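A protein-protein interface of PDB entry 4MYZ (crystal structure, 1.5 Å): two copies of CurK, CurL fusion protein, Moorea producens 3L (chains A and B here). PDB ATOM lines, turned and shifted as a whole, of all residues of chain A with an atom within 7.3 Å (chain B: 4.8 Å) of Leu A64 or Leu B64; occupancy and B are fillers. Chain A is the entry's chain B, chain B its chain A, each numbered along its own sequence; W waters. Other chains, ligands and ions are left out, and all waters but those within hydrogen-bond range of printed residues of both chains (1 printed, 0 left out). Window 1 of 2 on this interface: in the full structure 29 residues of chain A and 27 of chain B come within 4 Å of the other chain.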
ATOM      1  N   SER A  21       9.198  -8.141 -25.541  1.00  0.00           N
ATOM      2  CA  SER A  21       8.880  -9.447 -25.003  1.00  0.00           C
ATOM      3  C   SER A  21      10.155 -10.210 -24.604  1.00  0.00           C
ATOM      4  O   SER A  21      10.178 -10.902 -23.580  1.00  0.00           O
ATOM      5  CB  SER A  21       8.099 -10.260 -26.017  1.00  0.00           C
ATOM      6  OG  SER A  21       6.792  -9.718 -26.217  1.00  0.00           O
ATOM      7  N   VAL A  22      11.198 -10.111 -25.426  1.00  0.00           N
ATOM      8  CA  VAL A  22      12.485 -10.694 -25.098  1.00  0.00           C
ATOM      9  C   VAL A  22      12.994 -10.110 -23.771  1.00  0.00           C
ATOM     10  O   VAL A  22      13.467 -10.827 -22.894  1.00  0.00           O
ATOM     11  CB  VAL A  22      13.459 -10.482 -26.261  1.00  0.00           C
ATOM     12  CG1 VAL A  22      14.908 -10.686 -25.837  1.00  0.00           C
ATOM     13  CG2 VAL A  22      13.081 -11.419 -27.387  1.00  0.00           C
ATOM     14  N   LEU A  23      12.936  -8.798 -23.636  1.00  0.00           N
ATOM     15  CA  LEU A  23      13.429  -8.159 -22.415  1.00  0.00           C
ATOM     16  C   LEU A  23      12.647  -8.609 -21.179  1.00  0.00           C
ATOM     17  O   LEU A  23      13.215  -8.866 -20.113  1.00  0.00           O
ATOM     18  CB  LEU A  23      13.429  -6.639 -22.544  1.00  0.00           C
ATOM     19  CG  LEU A  23      14.415  -6.094 -23.552  1.00  0.00           C
ATOM     20  CD1 LEU A  23      14.173  -4.615 -23.808  1.00  0.00           C
ATOM     21  CD2 LEU A  23      15.842  -6.263 -23.068  1.00  0.00           C
ATOM     22  N   GLU A  25      11.193 -11.496 -20.819  1.00  0.00           N
ATOM     23  CA  GLU A  25      11.620 -12.842 -20.498  1.00  0.00           C
ATOM     24  C   GLU A  25      12.982 -12.866 -19.825  1.00  0.00           C
ATOM     25  O   GLU A  25      13.190 -13.659 -18.911  1.00  0.00           O
ATOM     26  CB  GLU A  25      11.633 -13.740 -21.726  1.00  0.00           C
ATOM     27  CG  GLU A  25      11.391 -15.191 -21.407  1.00  0.00           C
ATOM     28  CD  GLU A  25       9.982 -15.469 -20.871  1.00  0.00           C
ATOM     29  OE1 GLU A  25       9.855 -16.420 -20.108  1.00  0.00           O
ATOM     30  OE2 GLU A  25       9.010 -14.765 -21.240  1.00  0.00           O
ATOM     31  N   ILE A  26      13.893 -11.987 -20.257  1.00  0.00           N
ATOM     32  CA  ILE A  26      15.219 -11.904 -19.631  1.00  0.00           C
ATOM     33  C   ILE A  26      15.109 -11.491 -18.159  1.00  0.00           C
ATOM     34  O   ILE A  26      15.790 -12.049 -17.293  1.00  0.00           O
ATOM     35  CB  ILE A  26      16.137 -10.946 -20.404  1.00  0.00           C
ATOM     36  CG1 ILE A  26      16.456 -11.515 -21.788  1.00  0.00           C
ATOM     37  CG2 ILE A  26      17.409 -10.714 -19.638  1.00  0.00           C
ATOM     38  CD1 ILE A  26      17.167 -10.571 -22.703  1.00  0.00           C
ATOM     39  N   LEU A  29      14.025 -14.476 -16.180  1.00  0.00           N
ATOM     40  CA  LEU A  29      15.125 -15.424 -16.082  1.00  0.00           C
ATOM     41  C   LEU A  29      16.169 -14.956 -15.085  1.00  0.00           C
ATOM     42  O   LEU A  29      16.711 -15.776 -14.334  1.00  0.00           O
ATOM     43  CB  LEU A  29      15.727 -15.619 -17.468  1.00  0.00           C
ATOM     44  CG  LEU A  29      16.831 -16.606 -17.759  1.00  0.00           C
ATOM     45  CD1 LEU A  29      16.324 -18.002 -17.482  1.00  0.00           C
ATOM     46  CD2 LEU A  29      17.236 -16.455 -19.213  1.00  0.00           C
ATOM     47  N   ILE A  33      18.073 -17.089 -12.039  1.00  0.00           N
ATOM     48  CA  ILE A  33      19.511 -17.346 -12.020  1.00  0.00           C
ATOM     49  C   ILE A  33      20.144 -16.365 -11.052  1.00  0.00           C
ATOM     50  O   ILE A  33      21.123 -16.688 -10.395  1.00  0.00           O
ATOM     51  CB  ILE A  33      20.174 -17.111 -13.408  1.00  0.00           C
ATOM     52  CG1 ILE A  33      19.530 -17.982 -14.491  1.00  0.00           C
ATOM     53  CG2 ILE A  33      21.678 -17.383 -13.335  1.00  0.00           C
ATOM     54  CD1 ILE A  33      20.186 -17.865 -15.848  1.00  0.00           C
ATOM     55  N   ALA A  56      18.185  -5.542 -27.311  1.00  0.00           N
ATOM     56  CA  ALA A  56      17.539  -6.768 -26.846  1.00  0.00           C
ATOM     57  C   ALA A  56      18.275  -8.030 -27.303  1.00  0.00           C
ATOM     58  O   ALA A  56      18.402  -8.972 -26.546  1.00  0.00           O
ATOM     59  CB  ALA A  56      16.083  -6.817 -27.303  1.00  0.00           C
ATOM     60  N   LEU A  57      18.758  -8.052 -28.538  1.00  0.00           N
ATOM     61  CA  LEU A  57      19.433  -9.240 -29.032  1.00  0.00           C
ATOM     62  C   LEU A  57      20.759  -9.458 -28.302  1.00  0.00           C
ATOM     63  O   LEU A  57      21.145 -10.577 -28.021  1.00  0.00           O
ATOM     64  CB  LEU A  57      19.648  -9.170 -30.564  1.00  0.00           C
ATOM     65  CG  LEU A  57      20.161 -10.471 -31.212  1.00  0.00           C
ATOM     66  CD1 LEU A  57      19.241 -11.636 -30.983  1.00  0.00           C
ATOM     67  CD2 LEU A  57      20.362 -10.166 -32.715  1.00  0.00           C
ATOM     68  N   GLN A  58      21.468  -8.381 -28.009  1.00  0.00           N
ATOM     69  CA  GLN A  58      22.707  -8.479 -27.221  1.00  0.00           C
ATOM     70  C   GLN A  58      22.401  -9.003 -25.833  1.00  0.00           C
ATOM     71  O   GLN A  58      23.119  -9.880 -25.316  1.00  0.00           O
ATOM     72  CB  GLN A  58      23.405  -7.123 -27.133  1.00  0.00           C
ATOM     73  CG  GLN A  58      24.112  -6.745 -28.443  1.00  0.00           C
ATOM     74  CD  GLN A  58      24.594  -5.308 -28.474  1.00  0.00           C
ATOM     75  OE1 GLN A  58      23.990  -4.412 -27.917  1.00  0.00           O
ATOM     76  NE2 GLN A  58      25.648  -5.079 -29.268  1.00  0.00           N
ATOM     77  N   ARG A  59      21.380  -8.428 -25.187  1.00  0.00           N
ATOM     78  CA  ARG A  59      20.995  -8.939 -23.880  1.00  0.00           C
ATOM     79  C   ARG A  59      20.555 -10.403 -23.937  1.00  0.00           C
ATOM     80  O   ARG A  59      20.799 -11.171 -23.007  1.00  0.00           O
ATOM     81  CB  ARG A  59      19.927  -8.079 -23.223  1.00  0.00           C
ATOM     82  CG  ARG A  59      20.350  -6.679 -22.877  1.00  0.00           C
ATOM     83  CD  ARG A  59      19.393  -6.134 -21.842  1.00  0.00           C
ATOM     84  NE  ARG A  59      19.645  -4.759 -21.426  1.00  0.00           N
ATOM     85  CZ  ARG A  59      20.487  -4.396 -20.476  1.00  0.00           C
ATOM     86  NH1 ARG A  59      21.251  -5.284 -19.863  1.00  0.00           N
ATOM     87  NH2 ARG A  59      20.548  -3.113 -20.127  1.00  0.00           N
ATOM     88  N   ALA A  60      19.901 -10.787 -25.027  1.00  0.00           N
ATOM     89  CA  ALA A  60      19.460 -12.176 -25.201  1.00  0.00           C
ATOM     90  C   ALA A  60      20.643 -13.097 -25.252  1.00  0.00           C
ATOM     91  O   ALA A  60      20.579 -14.175 -24.668  1.00  0.00           O
ATOM     92  CB  ALA A  60      18.613 -12.350 -26.424  1.00  0.00           C
ATOM     93  N   LEU A  61      21.715 -12.734 -25.946  1.00  0.00           N
ATOM     94  CA  LEU A  61      22.895 -13.595 -25.993  1.00  0.00           C
ATOM     95  C   LEU A  61      23.441 -13.821 -24.583  1.00  0.00           C
ATOM     96  O   LEU A  61      23.777 -14.929 -24.209  1.00  0.00           O
ATOM     97  CB  LEU A  61      23.961 -12.986 -26.907  1.00  0.00           C
ATOM     98  CG  LEU A  61      25.264 -13.779 -26.993  1.00  0.00           C
ATOM     99  CD1 LEU A  61      25.004 -15.211 -27.402  1.00  0.00           C
ATOM    100  CD2 LEU A  61      26.238 -13.065 -27.918  1.00  0.00           C
ATOM    101  N   ILE A  62      23.563 -12.728 -23.827  1.00  0.00           N
ATOM    102  CA  ILE A  62      24.100 -12.840 -22.449  1.00  0.00           C
ATOM    103  C   ILE A  62      23.194 -13.764 -21.612  1.00  0.00           C
ATOM    104  O   ILE A  62      23.692 -14.648 -20.903  1.00  0.00           O
ATOM    105  CB  ILE A  62      24.240 -11.447 -21.821  1.00  0.00           C
ATOM    106  CG1 ILE A  62      25.342 -10.666 -22.534  1.00  0.00           C
ATOM    107  CG2 ILE A  62      24.520 -11.535 -20.341  1.00  0.00           C
ATOM    108  CD1 ILE A  62      25.348  -9.194 -22.235  1.00  0.00           C
ATOM    109  N   ALA A  63      21.885 -13.584 -21.718  1.00  0.00           N
ATOM    110  CA  ALA A  63      20.940 -14.347 -20.917  1.00  0.00           C
ATOM    111  C   ALA A  63      20.945 -15.815 -21.317  1.00  0.00           C
ATOM    112  O   ALA A  63      20.834 -16.692 -20.434  1.00  0.00           O
ATOM    113  CB  ALA A  63      19.550 -13.763 -21.088  1.00  0.00           C
ATOM    114  N   LEU A  64      21.041 -16.101 -22.609  1.00  0.00           N
ATOM    115  CA  LEU A  64      21.094 -17.489 -23.089  1.00  0.00           C
ATOM    116  C   LEU A  64      22.349 -18.169 -22.581  1.00  0.00           C
ATOM    117  O   LEU A  64      22.317 -19.354 -22.168  1.00  0.00           O
ATOM    118  CB  LEU A  64      20.992 -17.556 -24.631  1.00  0.00           C
ATOM    119  CG  LEU A  64      19.626 -17.177 -25.190  1.00  0.00           C
ATOM    120  CD1 LEU A  64      19.771 -16.837 -26.667  1.00  0.00           C
ATOM    121  CD2 LEU A  64      18.614 -18.283 -24.923  1.00  0.00           C
ATOM    122  N   LYS A  65      23.463 -17.458 -22.616  1.00  0.00           N
ATOM    123  CA  LYS A  65      24.723 -17.998 -22.121  1.00  0.00           C
ATOM    124  C   LYS A  65      24.624 -18.290 -20.631  1.00  0.00           C
ATOM    125  O   LYS A  65      25.105 -19.344 -20.166  1.00  0.00           O
ATOM    126  CB  LYS A  65      25.888 -17.068 -22.394  1.00  0.00           C
ATOM    127  CG  LYS A  65      26.321 -17.016 -23.844  1.00  0.00           C
ATOM    128  CD  LYS A  65      27.436 -15.992 -24.017  1.00  0.00           C
ATOM    129  CE  LYS A  65      28.783 -16.534 -23.592  1.00  0.00           C
ATOM    130  NZ  LYS A  65      29.364 -17.433 -24.631  1.00  0.00           N
ATOM    131  N   ASP A  66      24.038 -17.370 -19.878  1.00  0.00           N
ATOM    132  CA  ASP A  66      23.860 -17.569 -18.434  1.00  0.00           C
ATOM    133  C   ASP A  66      22.960 -18.788 -18.177  1.00  0.00           C
ATOM    134  O   ASP A  66      23.245 -19.614 -17.291  1.00  0.00           O
ATOM    135  CB  ASP A  66      23.259 -16.337 -17.763  1.00  0.00           C
ATOM    136  CG  ASP A  66      24.231 -15.156 -17.679  1.00  0.00           C
ATOM    137  OD1 ASP A  66      25.454 -15.373 -17.767  1.00  0.00           O
ATOM    138  OD2 ASP A  66      23.727 -14.014 -17.544  1.00  0.00           O
ATOM    139  N   ALA A  67      21.855 -18.905 -18.898  1.00  0.00           N
ATOM    140  CA  ALA A  67      20.942 -20.049 -18.723  1.00  0.00           C
ATOM    141  C   ALA A  67      21.660 -21.347 -19.054  1.00  0.00           C
ATOM    142  O   ALA A  67      21.518 -22.326 -18.329  1.00  0.00           O
ATOM    143  CB  ALA A  67      19.709 -19.901 -19.583  1.00  0.00           C
ATOM    144  N   ARG A  68      22.414 -21.371 -20.143  1.00  0.00           N
ATOM    145  CA  ARG A  68      23.145 -22.595 -20.545  1.00  0.00           C
ATOM    146  C   ARG A  68      24.171 -22.968 -19.491  1.00  0.00           C
ATOM    147  O   ARG A  68      24.281 -24.148 -19.115  1.00  0.00           O
ATOM    148  CB  ARG A  68      23.838 -22.391 -21.908  1.00  0.00           C
ATOM    149  CG  ARG A  68      24.687 -23.609 -22.351  1.00  0.00           C
ATOM    150  CD  ARG A  68      25.596 -23.242 -23.507  1.00  0.00           C
ATOM    151  NE  ARG A  68      26.541 -24.308 -23.840  1.00  0.00           N
ATOM    152  CZ  ARG A  68      27.361 -24.264 -24.888  1.00  0.00           C
ATOM    153  NH1 ARG A  68      28.174 -25.291 -25.130  1.00  0.00           N
ATOM    154  NH2 ARG A  68      27.366 -23.206 -25.703  1.00  0.00           N
ATOM    155  N   SER A  69      24.892 -22.005 -18.956  1.00  0.00           N
ATOM    156  CA  SER A  69      25.914 -22.284 -17.961  1.00  0.00           C
ATOM    157  C   SER A  69      25.302 -22.912 -16.732  1.00  0.00           C
ATOM    158  O   SER A  69      25.857 -23.876 -16.180  1.00  0.00           O
ATOM    159  CB  SER A  69      26.674 -21.040 -17.580  1.00  0.00           C
ATOM    160  OG  SER A  69      27.450 -20.601 -18.679  1.00  0.00           O
ATOM    161  N   LYS A  70      24.162 -22.415 -16.302  1.00  0.00           N
ATOM    162  CA  LYS A  70      23.526 -23.003 -15.138  1.00  0.00           C
ATOM    163  C   LYS A  70      22.958 -24.399 -15.455  1.00  0.00           C
ATOM    164  O   LYS A  70      23.134 -25.373 -14.679  1.00  0.00           O
ATOM    165  CB  LYS A  70      22.429 -22.106 -14.612  1.00  0.00           C
ATOM    166  CG  LYS A  70      21.759 -22.715 -13.395  1.00  0.00           C
ATOM    167  CD  LYS A  70      21.031 -21.701 -12.560  1.00  0.00           C
ATOM    168  CE  LYS A  70      20.334 -22.396 -11.409  1.00  0.00           C
ATOM    169  NZ  LYS A  70      20.650 -21.743 -10.127  1.00  0.00           N
ATOM    170  N   LEU A  71      22.266 -24.531 -16.571  1.00  0.00           N
ATOM    171  CA  LEU A  71      21.629 -25.803 -16.907  1.00  0.00           C
ATOM    172  C   LEU A  71      22.630 -26.915 -17.120  1.00  0.00           C
ATOM    173  O   LEU A  71      22.338 -28.096 -16.807  1.00  0.00           O
ATOM    174  CB  LEU A  71      20.714 -25.660 -18.114  1.00  0.00           C
ATOM    175  CG  LEU A  71      19.414 -24.923 -17.825  1.00  0.00           C
ATOM    176  CD1 LEU A  71      18.786 -24.461 -19.131  1.00  0.00           C
ATOM    177  CD2 LEU A  71      18.443 -25.781 -17.010  1.00  0.00           C
ATOM    178  N   VAL B  22      23.969 -16.256 -31.041  1.00  0.00           N
ATOM    179  CA  VAL B  22      22.672 -16.564 -30.437  1.00  0.00           C
ATOM    180  C   VAL B  22      22.204 -17.950 -30.883  1.00  0.00           C
ATOM    181  O   VAL B  22      21.804 -18.758 -30.052  1.00  0.00           O
ATOM    182  CB  VAL B  22      21.647 -15.467 -30.764  1.00  0.00           C
ATOM    183  CG1 VAL B  22      20.231 -15.950 -30.502  1.00  0.00           C
ATOM    184  CG2 VAL B  22      21.950 -14.182 -30.036  1.00  0.00           C
ATOM    185  N   GLU B  25      24.075 -20.716 -29.136  1.00  0.00           N
ATOM    186  CA  GLU B  25      23.601 -20.946 -27.763  1.00  0.00           C
ATOM    187  C   GLU B  25      22.277 -21.686 -27.721  1.00  0.00           C
ATOM    188  O   GLU B  25      22.057 -22.558 -26.872  1.00  0.00           O
ATOM    189  CB  GLU B  25      23.478 -19.623 -27.012  1.00  0.00           C
ATOM    190  CG  GLU B  25      24.810 -19.005 -26.677  1.00  0.00           C
ATOM    191  CD  GLU B  25      25.776 -19.903 -25.931  1.00  0.00           C
ATOM    192  OE1 GLU B  25      25.397 -20.608 -24.977  1.00  0.00           O
ATOM    193  OE2 GLU B  25      26.949 -19.867 -26.295  1.00  0.00           O
ATOM    194  N   ILE B  26      21.399 -21.347 -28.660  1.00  0.00           N
ATOM    195  CA  ILE B  26      20.116 -22.006 -28.755  1.00  0.00           C
ATOM    196  C   ILE B  26      20.297 -23.478 -29.093  1.00  0.00           C
ATOM    197  O   ILE B  26      19.608 -24.322 -28.512  1.00  0.00           O
ATOM    198  CB  ILE B  26      19.198 -21.285 -29.740  1.00  0.00           C
ATOM    199  CG1 ILE B  26      18.900 -19.877 -29.211  1.00  0.00           C
ATOM    200  CG2 ILE B  26      17.909 -22.053 -29.937  1.00  0.00           C
ATOM    201  CD1 ILE B  26      18.077 -19.044 -30.149  1.00  0.00           C
ATOM    202  N   LEU B  29      21.462 -25.234 -25.956  1.00  0.00           N
ATOM    203  CA  LEU B  29      20.332 -25.418 -25.053  1.00  0.00           C
ATOM    204  C   LEU B  29      19.398 -26.538 -25.502  1.00  0.00           C
ATOM    205  O   LEU B  29      18.923 -27.292 -24.650  1.00  0.00           O
ATOM    206  CB  LEU B  29      19.517 -24.132 -24.887  1.00  0.00           C
ATOM    207  CG  LEU B  29      20.191 -23.102 -23.984  1.00  0.00           C
ATOM    208  CD1 LEU B  29      19.685 -21.687 -24.210  1.00  0.00           C
ATOM    209  CD2 LEU B  29      19.987 -23.447 -22.526  1.00  0.00           C
ATOM    210  N   ALA B  60      15.272 -16.583 -30.215  1.00  0.00           N
ATOM    211  CA  ALA B  60      15.728 -16.275 -28.855  1.00  0.00           C
ATOM    212  C   ALA B  60      14.574 -16.169 -27.888  1.00  0.00           C
ATOM    213  O   ALA B  60      14.680 -16.666 -26.767  1.00  0.00           O
ATOM    214  CB  ALA B  60      16.554 -14.984 -28.840  1.00  0.00           C
ATOM    215  N   LEU B  61      13.471 -15.537 -28.299  1.00  0.00           N
ATOM    216  CA  LEU B  61      12.317 -15.427 -27.404  1.00  0.00           C
ATOM    217  C   LEU B  61      11.810 -16.831 -27.004  1.00  0.00           C
ATOM    218  O   LEU B  61      11.535 -17.123 -25.823  1.00  0.00           O
ATOM    219  CB  LEU B  61      11.196 -14.591 -28.035  1.00  0.00           C
ATOM    220  CG  LEU B  61       9.931 -14.507 -27.200  1.00  0.00           C
ATOM    221  CD1 LEU B  61      10.221 -13.894 -25.829  1.00  0.00           C
ATOM    222  CD2 LEU B  61       8.874 -13.718 -27.937  1.00  0.00           C
ATOM    223  N   ILE B  62      11.694 -17.707 -28.000  1.00  0.00           N
ATOM    224  CA  ILE B  62      11.251 -19.075 -27.762  1.00  0.00           C
ATOM    225  C   ILE B  62      12.216 -19.797 -26.827  1.00  0.00           C
ATOM    226  O   ILE B  62      11.796 -20.455 -25.873  1.00  0.00           O
ATOM    227  CB  ILE B  62      11.087 -19.841 -29.103  1.00  0.00           C
ATOM    228  CG1 ILE B  62       9.939 -19.239 -29.917  1.00  0.00           C
ATOM    229  CG2 ILE B  62      10.842 -21.330 -28.865  1.00  0.00           C
ATOM    230  CD1 ILE B  62       9.914 -19.733 -31.346  1.00  0.00           C
ATOM    231  N   ALA B  63      13.501 -19.671 -27.097  1.00  0.00           N
ATOM    232  CA  ALA B  63      14.519 -20.341 -26.294  1.00  0.00           C
ATOM    233  C   ALA B  63      14.577 -19.808 -24.862  1.00  0.00           C
ATOM    234  O   ALA B  63      14.788 -20.589 -23.913  1.00  0.00           O
ATOM    235  CB  ALA B  63      15.882 -20.215 -26.951  1.00  0.00           C
ATOM    236  N   LEU B  64      14.415 -18.512 -24.688  1.00  0.00           N
ATOM    237  CA  LEU B  64      14.390 -17.928 -23.336  1.00  0.00           C
ATOM    238  C   LEU B  64      13.187 -18.429 -22.534  1.00  0.00           C
ATOM    239  O   LEU B  64      13.329 -18.703 -21.340  1.00  0.00           O
ATOM    240  CB  LEU B  64      14.425 -16.397 -23.423  1.00  0.00           C
ATOM    241  CG  LEU B  64      15.718 -15.727 -23.912  1.00  0.00           C
ATOM    242  CD1 LEU B  64      15.434 -14.309 -24.392  1.00  0.00           C
ATOM    243  CD2 LEU B  64      16.753 -15.702 -22.788  1.00  0.00           C
ATOM    244  N   LYS B  65      12.013 -18.517 -23.166  1.00  0.00           N
ATOM    245  CA  LYS B  65      10.826 -19.025 -22.485  1.00  0.00           C
ATOM    246  C   LYS B  65      11.049 -20.468 -22.074  1.00  0.00           C
ATOM    247  O   LYS B  65      10.740 -20.846 -20.946  1.00  0.00           O
ATOM    248  CB  LYS B  65       9.593 -18.919 -23.366  1.00  0.00           C
ATOM    249  CG  LYS B  65       9.077 -17.500 -23.550  1.00  0.00           C
ATOM    250  CD  LYS B  65       8.031 -17.459 -24.655  1.00  0.00           C
ATOM    251  CE  LYS B  65       7.292 -16.131 -24.698  1.00  0.00           C
ATOM    252  NZ  LYS B  65       6.347 -16.034 -23.562  1.00  0.00           N
ATOM    253  N   ASP B  66      11.633 -21.265 -22.963  1.00  0.00           N
ATOM    254  CA  ASP B  66      11.902 -22.684 -22.659  1.00  0.00           C
ATOM    255  C   ASP B  66      12.926 -22.827 -21.543  1.00  0.00           C
ATOM    256  O   ASP B  66      12.745 -23.661 -20.634  1.00  0.00           O
ATOM    257  CB  ASP B  66      12.430 -23.420 -23.897  1.00  0.00           C
ATOM    258  CG  ASP B  66      11.384 -23.624 -24.955  1.00  0.00           C
ATOM    259  OD1 ASP B  66      10.177 -23.643 -24.617  1.00  0.00           O
ATOM    260  OD2 ASP B  66      11.768 -23.781 -26.148  1.00  0.00           O
ATOM    261  N   ALA B  67      14.011 -22.068 -21.622  1.00  0.00           N
ATOM    262  CA  ALA B  67      15.050 -22.103 -20.584  1.00  0.00           C
ATOM    263  C   ALA B  67      14.483 -21.675 -19.235  1.00  0.00           C
ATOM    264  O   ALA B  67      14.764 -22.323 -18.210  1.00  0.00           O
ATOM    265  CB  ALA B  67      16.251 -21.258 -20.974  1.00  0.00           C
ATOM    266  N   ARG B  68      13.666 -20.631 -19.215  1.00  0.00           N
ATOM    267  CA  ARG B  68      13.033 -20.175 -17.967  1.00  0.00           C
ATOM    268  C   ARG B  68      12.187 -21.260 -17.355  1.00  0.00           C
ATOM    269  O   ARG B  68      12.279 -21.530 -16.144  1.00  0.00           O
ATOM    270  CB  ARG B  68      12.175 -18.923 -18.224  1.00  0.00           C
ATOM    271  CG  ARG B  68      11.405 -18.392 -17.022  1.00  0.00           C
ATOM    272  CD  ARG B  68      10.388 -17.352 -17.486  1.00  0.00           C
ATOM    273  NE  ARG B  68       9.468 -16.955 -16.422  1.00  0.00           N
ATOM    274  CZ  ARG B  68       8.411 -16.168 -16.596  1.00  0.00           C
ATOM    275  NH1 ARG B  68       8.109 -15.691 -17.802  1.00  0.00           N
ATOM    276  NH2 ARG B  68       7.647 -15.859 -15.552  1.00  0.00           N
HETATM  277  O   HOH W   1       7.494 -17.498 -20.238  1.00  0.00           O
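Of the printed residues of chain B, Leu A64 touches Val B22, Leu B29, Ala B63 and Leu B64. Leu B64 touches six residues of chain A. Ala B63 touches just one residue of chain A: Leu A64. Of the printed residues of chain B, Leu A71 touches Leu B29. Printed residues of chain B within 4 Å of Leu A61: Val B22 (3.9 Å) and Glu B25 (3.9 Å). Of the printed residues of chain B, Arg A68 touches Glu B25 (3.0 Å) and Leu B29 (3.8 Å). Of the printed residues of chain A, Lys B65 touches Glu A25 (3.5 Å). Leu A23 touches none of the printed residues of chain B. Ala A60 touches none of the printed residues of chain B. The nearest printed residue of chain B that does not touch Leu A57 is Ala B60 (4.8 Å).
The side-chain hydroxyl (OG) of Ser A69 is in hydrogen-bond range of the backbone carbonyl oxygen (O) of Lys A65 (3.0 Å).
Among the printed residues, merely in contact across the chains: Leu A64 with Leu B29 (3.6 Å), Leu A29 with Leu B64 (3.7 Å), Leu A71 with Leu B29 (3.7 Å), Ser A21 with Leu B61 (3.7 Å), Val A22 with Leu B61 (3.7 Å), Ala A63 with Leu B64 (3.8 Å), Arg A68 with Leu B29 (3.8 Å), Leu A64 with Leu B64 (3.8 Å), Leu A57 with Val B22 (3.8 Å), Glu A25 with Leu B64 (3.8 Å), Leu A61 with Glu B25 (3.9 Å), Leu A61 with Val B22 (3.9 Å), Leu A64 with Ala B63 (3.9 Å), Val A22 with Leu B64 (3.9 Å), Ile A26 with Leu B64 (3.95 Å), Leu A64 with Val B22 (3.96 Å), Ala A67 with Ala B67 (3.97 Å) and Leu A29 with Arg B68 (3.97 Å).
NH1 of Arg B68 is in salt-bridge range of OE1 of Glu A25, at 3.0 Å. OE2 of Glu B25 is in salt-bridge range of NZ of Lys A65 (3.8 Å). The side-chain amino group (NZ) of Lys B65 lies within salt-bridge range of the side-chain carboxylate (OE2) of Glu A25 (3.8 Å). The side-chain carboxylate (OE1) of Glu B25 lies within salt-bridge range of the guanidinium group (NH2) of Arg A68 (3.3 Å).
Glu A25 touches Leu B64, but with the chains exchanged Leu A64 does not touch Glu B25 (4.02 Å). Leu A29 touches Arg B68, and with the chains exchanged Arg A68 touches Leu B29. Leu A61 touches Glu B25, but with the chains exchanged Glu A25 does not touch Leu B61 (4.3 Å). Leu B64 touches its own counterpart, Leu A64.
Hydrophobic or aromatic side chains of chain A that line the printed part of chain B: Val A22, Ile A26, Leu A29, Leu A57, Leu A61, Ala A63, Leu A64, Ala A67 and Leu A71. Of the 13 printed residues of chain B, 9 touch a printed residue of chain A. Among the printed residues, 22 pairs touch across the chains. Among the printed residues, Asp or Glu carboxylates within 4 Å of a Lys or Arg side-chain nitrogen of the other chain: Glu A25 with Lys B65 (3.8 Å), Glu A25 with Arg B68 (3.0 Å), Lys A65 with Glu B25 (3.8 Å) and Arg A68 with Glu B25 (3.3 Å).
Water W1 bridges OE1 of Glu A25 (2.6 Å) and NH1 of Arg B68 (3.1 Å).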
